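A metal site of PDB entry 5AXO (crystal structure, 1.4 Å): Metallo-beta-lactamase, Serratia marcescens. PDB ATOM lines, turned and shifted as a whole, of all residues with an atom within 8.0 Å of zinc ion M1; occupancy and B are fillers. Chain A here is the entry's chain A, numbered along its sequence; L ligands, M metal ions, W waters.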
ATOM      1  N   TRP A   5      10.848 -20.881  -5.875  1.00  0.00           N
ATOM      2  CA  TRP A   5      11.191 -19.474  -6.158  1.00  0.00           C
ATOM      3  C   TRP A   5      12.667 -19.159  -5.837  1.00  0.00           C
ATOM      4  O   TRP A   5      13.242 -18.220  -6.396  1.00  0.00           O
ATOM      5  CB  TRP A   5      10.379 -18.495  -5.310  1.00  0.00           C
ATOM      6  CG  TRP A   5       8.958 -18.373  -5.610  1.00  0.00           C
ATOM      7  CD1 TRP A   5       8.291 -18.897  -6.655  1.00  0.00           C
ATOM      8  CD2 TRP A   5       7.993 -17.734  -4.775  1.00  0.00           C
ATOM      9  NE1 TRP A   5       6.956 -18.548  -6.580  1.00  0.00           N
ATOM     10  CE2 TRP A   5       6.761 -17.837  -5.430  1.00  0.00           C
ATOM     11  CE3 TRP A   5       8.055 -17.020  -3.567  1.00  0.00           C
ATOM     12  CZ2 TRP A   5       5.569 -17.332  -4.878  1.00  0.00           C
ATOM     13  CZ3 TRP A   5       6.880 -16.530  -3.014  1.00  0.00           C
ATOM     14  CH2 TRP A   5       5.681 -16.639  -3.700  1.00  0.00           C
ATOM     15  N   THR A  71      10.406  -5.418 -12.432  1.00  0.00           N
ATOM     16  CA  THR A  71       9.106  -5.597 -13.010  1.00  0.00           C
ATOM     17  C   THR A  71       7.987  -5.169 -12.081  1.00  0.00           C
ATOM     18  O   THR A  71       7.245  -4.184 -12.399  1.00  0.00           O
ATOM     19  CB  THR A  71       8.870  -7.049 -13.463  1.00  0.00           C
ATOM     20  OG1 THR A  71       9.059  -7.913 -12.373  1.00  0.00           O
ATOM     21  CG2 THR A  71       9.726  -7.435 -14.652  1.00  0.00           C
ATOM     22  N   HIS A  72       7.822  -5.856 -10.967  1.00  0.00           N
ATOM     23  CA  HIS A  72       6.889  -5.369  -9.964  1.00  0.00           C
ATOM     24  C   HIS A  72       7.256  -5.857  -8.578  1.00  0.00           C
ATOM     25  O   HIS A  72       8.094  -6.730  -8.357  1.00  0.00           O
ATOM     26  CB  HIS A  72       5.446  -5.813 -10.352  1.00  0.00           C
ATOM     27  CG  HIS A  72       5.164  -7.275 -10.107  1.00  0.00           C
ATOM     28  ND1 HIS A  72       5.317  -8.221 -11.093  1.00  0.00           N
ATOM     29  CD2 HIS A  72       4.707  -7.942  -9.022  1.00  0.00           C
ATOM     30  CE1 HIS A  72       4.993  -9.410 -10.608  1.00  0.00           C
ATOM     31  NE2 HIS A  72       4.602  -9.272  -9.362  1.00  0.00           N
ATOM     32  N   SER A  73       6.573  -5.243  -7.625  1.00  0.00           N
ATOM     33  CA  SER A  73       6.995  -5.198  -6.217  1.00  0.00           C
ATOM     34  C   SER A  73       6.286  -6.229  -5.353  1.00  0.00           C
ATOM     35  O   SER A  73       5.588  -5.874  -4.409  1.00  0.00           O
ATOM     36  CB  SER A  73       6.775  -3.804  -5.666  1.00  0.00           C
ATOM     37  OG  SER A  73       5.460  -3.346  -5.936  1.00  0.00           O
ATOM     38  N   HIS A  74       6.476  -7.513  -5.700  1.00  0.00           N
ATOM     39  CA  HIS A  74       6.076  -8.620  -4.803  1.00  0.00           C
ATOM     40  C   HIS A  74       7.319  -9.429  -4.397  1.00  0.00           C
ATOM     41  O   HIS A  74       8.346  -9.407  -5.116  1.00  0.00           O
ATOM     42  CB  HIS A  74       5.093  -9.543  -5.501  1.00  0.00           C
ATOM     43  CG  HIS A  74       3.765  -8.921  -5.734  1.00  0.00           C
ATOM     44  ND1 HIS A  74       2.922  -9.344  -6.745  1.00  0.00           N
ATOM     45  CD2 HIS A  74       3.113  -7.940  -5.071  1.00  0.00           C
ATOM     46  CE1 HIS A  74       1.799  -8.664  -6.660  1.00  0.00           C
ATOM     47  NE2 HIS A  74       1.897  -7.806  -5.659  1.00  0.00           N
ATOM     48  N   GLU A  75       7.212 -10.174  -3.299  1.00  0.00           N
ATOM     49  CA  GLU A  75       8.363 -10.831  -2.738  1.00  0.00           C
ATOM     50  C   GLU A  75       9.056 -11.764  -3.700  1.00  0.00           C
ATOM     51  O   GLU A  75      10.256 -11.987  -3.589  1.00  0.00           O
ATOM     52  CB  GLU A  75       7.961 -11.604  -1.477  1.00  0.00           C
ATOM     53  CG  GLU A  75       7.073 -12.821  -1.739  1.00  0.00           C
ATOM     54  CD  GLU A  75       6.713 -13.671  -0.523  1.00  0.00           C
ATOM     55  OE1 GLU A  75       7.577 -13.901   0.339  1.00  0.00           O
ATOM     56  OE2 GLU A  75       5.545 -14.128  -0.437  1.00  0.00           O
ATOM     57  N   ASP A  76       8.305 -12.427  -4.561  1.00  0.00           N
ATOM     58  CA  ASP A  76       8.890 -13.421  -5.466  1.00  0.00           C
ATOM     59  C   ASP A  76       9.817 -12.822  -6.553  1.00  0.00           C
ATOM     60  O   ASP A  76      10.763 -13.486  -6.925  1.00  0.00           O
ATOM     61  CB  ASP A  76       7.823 -14.367  -6.037  1.00  0.00           C
ATOM     62  CG  ASP A  76       6.669 -13.682  -6.719  1.00  0.00           C
ATOM     63  OD1 ASP A  76       6.230 -12.570  -6.311  1.00  0.00           O
ATOM     64  OD2 ASP A  76       6.134 -14.385  -7.570  1.00  0.00           O
ATOM     65  N   HIS A  77       9.544 -11.600  -7.007  1.00  0.00           N
ATOM     66  CA  HIS A  77      10.378 -10.927  -7.987  1.00  0.00           C
ATOM     67  C   HIS A  77      11.331  -9.927  -7.403  1.00  0.00           C
ATOM     68  O   HIS A  77      12.408  -9.651  -7.986  1.00  0.00           O
ATOM     69  CB  HIS A  77       9.472 -10.275  -9.020  1.00  0.00           C
ATOM     70  CG  HIS A  77       8.438 -11.189  -9.570  1.00  0.00           C
ATOM     71  ND1 HIS A  77       8.718 -12.145 -10.528  1.00  0.00           N
ATOM     72  CD2 HIS A  77       7.154 -11.402  -9.168  1.00  0.00           C
ATOM     73  CE1 HIS A  77       7.641 -12.892 -10.721  1.00  0.00           C
ATOM     74  NE2 HIS A  77       6.683 -12.473  -9.903  1.00  0.00           N
ATOM     75  N   ALA A  78      10.913  -9.246  -6.363  1.00  0.00           N
ATOM     76  CA  ALA A  78      11.578  -8.090  -5.778  1.00  0.00           C
ATOM     77  C   ALA A  78      12.237  -8.391  -4.443  1.00  0.00           C
ATOM     78  O   ALA A  78      12.978  -7.549  -3.898  1.00  0.00           O
ATOM     79  CB  ALA A  78      10.657  -6.911  -5.624  1.00  0.00           C
ATOM     80  N   SER A 107       3.391  -4.066   0.279  1.00  0.00           N
ATOM     81  CA  SER A 107       2.429  -3.732  -0.763  1.00  0.00           C
ATOM     82  C   SER A 107       1.206  -2.990  -0.182  1.00  0.00           C
ATOM     83  O   SER A 107       0.753  -3.344   0.895  1.00  0.00           O
ATOM     84  CB  SER A 107       2.004  -4.972  -1.565  1.00  0.00           C
ATOM     85  OG  SER A 107       3.058  -5.496  -2.360  1.00  0.00           O
ATOM     86  N   ASP A 111      -3.321  -2.975  -4.056  1.00  0.00           N
ATOM     87  CA  ASP A 111      -2.968  -4.270  -4.639  1.00  0.00           C
ATOM     88  C   ASP A 111      -4.087  -5.286  -4.438  1.00  0.00           C
ATOM     89  O   ASP A 111      -4.492  -5.544  -3.322  1.00  0.00           O
ATOM     90  CB  ASP A 111      -1.685  -4.760  -3.975  1.00  0.00           C
ATOM     91  CG  ASP A 111      -1.008  -5.904  -4.755  1.00  0.00           C
ATOM     92  OD1 ASP A 111      -1.667  -6.913  -5.012  1.00  0.00           O
ATOM     93  OD2 ASP A 111       0.179  -5.790  -5.054  1.00  0.00           O
ATOM     94  N   GLN A 113      -3.978  -8.340  -4.216  1.00  0.00           N
ATOM     95  CA  GLN A 113      -3.587  -9.373  -3.276  1.00  0.00           C
ATOM     96  C   GLN A 113      -3.401  -8.859  -1.837  1.00  0.00           C
ATOM     97  O   GLN A 113      -3.039  -9.657  -0.992  1.00  0.00           O
ATOM     98  CB  GLN A 113      -2.331 -10.090  -3.772  1.00  0.00           C
ATOM     99  CG  GLN A 113      -2.567 -10.889  -5.047  1.00  0.00           C
ATOM    100  CD  GLN A 113      -1.357 -11.697  -5.432  1.00  0.00           C
ATOM    101  OE1 GLN A 113      -1.102 -12.763  -4.866  1.00  0.00           O
ATOM    102  NE2 GLN A 113      -0.565 -11.195  -6.363  1.00  0.00           N
ATOM    103  N   LEU A 117      -0.404 -10.994   0.859  1.00  0.00           N
ATOM    104  CA  LEU A 117       1.005 -10.895   0.470  1.00  0.00           C
ATOM    105  C   LEU A 117       1.929 -10.945   1.666  1.00  0.00           C
ATOM    106  O   LEU A 117       1.594 -10.416   2.742  1.00  0.00           O
ATOM    107  CB  LEU A 117       1.232  -9.574  -0.283  1.00  0.00           C
ATOM    108  CG  LEU A 117       0.539  -9.524  -1.676  1.00  0.00           C
ATOM    109  CD1 LEU A 117       0.488  -8.092  -2.193  1.00  0.00           C
ATOM    110  CD2 LEU A 117       1.292 -10.359  -2.681  1.00  0.00           C
ATOM    111  N   HIS A 150      -1.505  -6.083 -12.402  1.00  0.00           N
ATOM    112  CA  HIS A 150      -1.101  -6.972 -11.350  1.00  0.00           C
ATOM    113  C   HIS A 150      -0.529  -6.135 -10.171  1.00  0.00           C
ATOM    114  O   HIS A 150      -0.743  -6.483  -8.998  1.00  0.00           O
ATOM    115  CB  HIS A 150      -0.072  -8.002 -11.911  1.00  0.00           C
ATOM    116  CG  HIS A 150       0.441  -8.996 -10.917  1.00  0.00           C
ATOM    117  ND1 HIS A 150      -0.212 -10.160 -10.588  1.00  0.00           N
ATOM    118  CD2 HIS A 150       1.632  -9.051 -10.253  1.00  0.00           C
ATOM    119  CE1 HIS A 150       0.569 -10.900  -9.833  1.00  0.00           C
ATOM    120  NE2 HIS A 150       1.623 -10.182  -9.492  1.00  0.00           N
ATOM    121  N   THR A 151       0.131  -5.017 -10.502  1.00  0.00           N
ATOM    122  CA  THR A 151       0.457  -3.975  -9.542  1.00  0.00           C
ATOM    123  C   THR A 151       0.309  -2.659 -10.321  1.00  0.00           C
ATOM    124  O   THR A 151       0.409  -2.616 -11.554  1.00  0.00           O
ATOM    125  CB  THR A 151       1.904  -4.058  -9.014  1.00  0.00           C
ATOM    126  OG1 THR A 151       2.825  -3.804 -10.075  1.00  0.00           O
ATOM    127  CG2 THR A 151       2.173  -5.343  -8.275  1.00  0.00           C
ATOM    128  N   ASP A 174       6.613  -8.410 -17.564  1.00  0.00           N
ATOM    129  CA  ASP A 174       5.993  -8.389 -16.267  1.00  0.00           C
ATOM    130  C   ASP A 174       4.787  -9.291 -16.265  1.00  0.00           C
ATOM    131  O   ASP A 174       4.210  -9.648 -17.312  1.00  0.00           O
ATOM    132  CB  ASP A 174       5.614  -6.965 -15.887  1.00  0.00           C
ATOM    133  CG  ASP A 174       5.256  -6.779 -14.410  1.00  0.00           C
ATOM    134  OD1 ASP A 174       5.601  -7.654 -13.622  1.00  0.00           O
ATOM    135  OD2 ASP A 174       4.587  -5.758 -14.117  1.00  0.00           O
ATOM    136  N   SER A 175       4.394  -9.682 -15.070  1.00  0.00           N
ATOM    137  CA  SER A 175       3.160 -10.446 -14.873  1.00  0.00           C
ATOM    138  C   SER A 175       1.927  -9.613 -15.213  1.00  0.00           C
ATOM    139  O   SER A 175       1.818  -8.472 -14.769  1.00  0.00           O
ATOM    140  CB  SER A 175       3.078 -10.914 -13.433  1.00  0.00           C
ATOM    141  OG  SER A 175       4.220 -11.713 -13.084  1.00  0.00           O
ATOM    142  N   LEU A 176       0.995 -10.229 -15.896  1.00  0.00           N
ATOM    143  CA  LEU A 176      -0.267  -9.603 -16.319  1.00  0.00           C
ATOM    144  C   LEU A 176      -1.463 -10.302 -15.671  1.00  0.00           C
ATOM    145  O   LEU A 176      -2.541 -10.330 -16.259  1.00  0.00           O
ATOM    146  CB  LEU A 176      -0.360  -9.679 -17.843  1.00  0.00           C
ATOM    147  CG  LEU A 176       0.783  -9.064 -18.635  1.00  0.00           C
ATOM    148  CD1 LEU A 176       0.544  -9.191 -20.114  1.00  0.00           C
ATOM    149  CD2 LEU A 176       1.074  -7.642 -18.239  1.00  0.00           C
ATOM    150  N   THR A 177      -1.249 -10.947 -14.524  1.00  0.00           N
ATOM    151  CA  THR A 177      -2.240 -11.847 -13.975  1.00  0.00           C
ATOM    152  C   THR A 177      -3.154 -11.223 -12.943  1.00  0.00           C
ATOM    153  O   THR A 177      -2.737 -10.570 -11.995  1.00  0.00           O
ATOM    154  CB  THR A 177      -1.506 -13.022 -13.308  1.00  0.00           C
ATOM    155  OG1 THR A 177      -0.602 -12.502 -12.340  1.00  0.00           O
ATOM    156  CG2 THR A 177      -0.790 -13.827 -14.348  1.00  0.00           C
ATOM    157  N   VAL A 179      -4.929 -11.851 -10.004  1.00  0.00           N
ATOM    158  CA  VAL A 179      -5.028 -12.679  -8.800  1.00  0.00           C
ATOM    159  C   VAL A 179      -5.341 -11.822  -7.616  1.00  0.00           C
ATOM    160  O   VAL A 179      -4.951 -10.691  -7.556  1.00  0.00           O
ATOM    161  CB  VAL A 179      -3.736 -13.439  -8.549  1.00  0.00           C
ATOM    162  CG1 VAL A 179      -3.535 -14.447  -9.641  1.00  0.00           C
ATOM    163  CG2 VAL A 179      -2.547 -12.555  -8.534  1.00  0.00           C
ATOM    164  N   ALA A 214       8.419 -13.063 -16.284  1.00  0.00           N
ATOM    165  CA  ALA A 214       8.846 -12.994 -14.877  1.00  0.00           C
ATOM    166  C   ALA A 214       8.773 -14.338 -14.128  1.00  0.00           C
ATOM    167  O   ALA A 214       9.697 -14.740 -13.405  1.00  0.00           O
ATOM    168  CB  ALA A 214       8.061 -11.909 -14.174  1.00  0.00           C
ATOM    169  N   HIS A 215       7.698 -15.061 -14.400  1.00  0.00           N
ATOM    170  CA  HIS A 215       7.614 -16.490 -14.072  1.00  0.00           C
ATOM    171  C   HIS A 215       7.997 -17.210 -15.361  1.00  0.00           C
ATOM    172  O   HIS A 215       7.261 -17.186 -16.310  1.00  0.00           O
ATOM    173  CB  HIS A 215       6.197 -16.901 -13.630  1.00  0.00           C
ATOM    174  CG  HIS A 215       5.860 -16.398 -12.262  1.00  0.00           C
ATOM    175  ND1 HIS A 215       6.193 -17.078 -11.120  1.00  0.00           N
ATOM    176  CD2 HIS A 215       5.330 -15.215 -11.871  1.00  0.00           C
ATOM    177  CE1 HIS A 215       5.896 -16.328 -10.067  1.00  0.00           C
ATOM    178  NE2 HIS A 215       5.385 -15.180 -10.494  1.00  0.00           N
HETATM  179  C1  LIG L   1       1.059 -16.098  -8.428  1.00  0.00           C
HETATM  180  C2  LIG L   1       0.925 -15.339  -9.758  1.00  0.00           C
HETATM  181  C3  LIG L   1       2.234 -14.581  -9.802  1.00  0.00           C
HETATM  182  O1  LIG L   1       1.138 -21.050 -11.393  1.00  0.00           O
HETATM  183  C4  LIG L   1       2.269 -20.667 -11.114  1.00  0.00           C
HETATM  184  N1  LIG L   1       3.076 -21.347 -10.313  1.00  0.00           N
HETATM  185  C5  LIG L   1       4.510 -21.086 -10.179  1.00  0.00           C
HETATM  186  C6  LIG L   1       2.633 -22.482  -9.511  1.00  0.00           C
HETATM  187  C7  LIG L   1       2.799 -19.399 -11.721  1.00  0.00           C
HETATM  188  C8  LIG L   1       2.523 -18.208 -10.820  1.00  0.00           C
HETATM  189  N2  LIG L   1       2.145 -19.110 -13.029  1.00  0.00           N
HETATM  190  C9  LIG L   1       2.035 -17.641 -13.169  1.00  0.00           C
HETATM  191  C10 LIG L   1       2.152 -17.058 -11.753  1.00  0.00           C
HETATM  192  S1  LIG L   1       0.628 -16.362 -11.231  1.00  0.00           S
HETATM  193  C11 LIG L   1       2.531 -13.659 -10.905  1.00  0.00           C
HETATM  194  O2  LIG L   1       1.795 -13.735 -11.925  1.00  0.00           O
HETATM  195  O3  LIG L   1       3.573 -12.822 -10.853  1.00  0.00           O
HETATM  196  N3  LIG L   1       2.981 -14.743  -8.798  1.00  0.00           N
HETATM  197  C12 LIG L   1      -0.120 -15.743  -7.490  1.00  0.00           C
HETATM  198  C13 LIG L   1       2.483 -15.764  -7.899  1.00  0.00           C
HETATM  199  C14 LIG L   1       2.707 -15.259  -6.449  1.00  0.00           C
HETATM  200  C15 LIG L   1       1.991 -13.952  -6.022  1.00  0.00           C
HETATM  201  O4  LIG L   1       1.711 -13.012  -7.059  1.00  0.00           O
HETATM  202  C16 LIG L   1       2.771 -13.193  -4.951  1.00  0.00           C
HETATM  203  C17 LIG L   1       2.295 -16.364  -5.526  1.00  0.00           C
HETATM  204  O5  LIG L   1       1.934 -16.153  -4.374  1.00  0.00           O
HETATM  205  O6  LIG L   1       2.442 -17.601  -5.944  1.00  0.00           O
HETATM  206 ZN    ZN M   1       3.357 -10.521  -8.363  1.00  0.00          ZN
HETATM  207 ZN    ZN M   2       4.983 -13.545  -9.234  1.00  0.00          ZN
HETATM  208  O   HOH W   1       4.087 -12.140  -7.999  1.00  0.00           O
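A ring nitrogen (ND1) of His 72 lies within hydrogen-bond range of the side-chain carboxylate (OD1) of Asp 174, 2.6 Å away. NE2 of His 74 lies within hydrogen-bond range of OD2 of Asp 111. The backbone carbonyl oxygen (O) of Thr 177 lies within hydrogen-bond range of a ring nitrogen (ND1) of His 150 (2.9 Å).
NE2 of Gln 113 is in hydrogen-bond range of O4 of the ligand (3.0 Å). The side-chain hydroxyl of Ser 175 lies within hydrogen-bond range of an oxygen (O2) of the ligand, 3.4 Å away. The side-chain hydroxyl of Thr 177 sits at hydrogen-bond distance from an oxygen (O2) of the ligand, at 2.7 Å.
CD2 of His 77 touches zinc ion M1 (3.98 Å). Within 4 Å of zinc ion M1: His 72, His 74, His 77 and His 150.
Water W1 lies within hydrogen-bond range of an oxygen (O4) of the ligand (2.7 Å) and the side-chain carboxylate of Asp 76 (2.8 Å).
Zinc ion M1 is bound by water W1, at 1.8 Å. NE2 of His 72 is bound to zinc ion M1. Zinc ion M1 is bound by ND1 of His 74 (2.0 Å). A ring nitrogen (NE2) of His 150 is bound to zinc ion M1 (2.1 Å). Zinc ion M1 has four donor atoms within binding distance.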
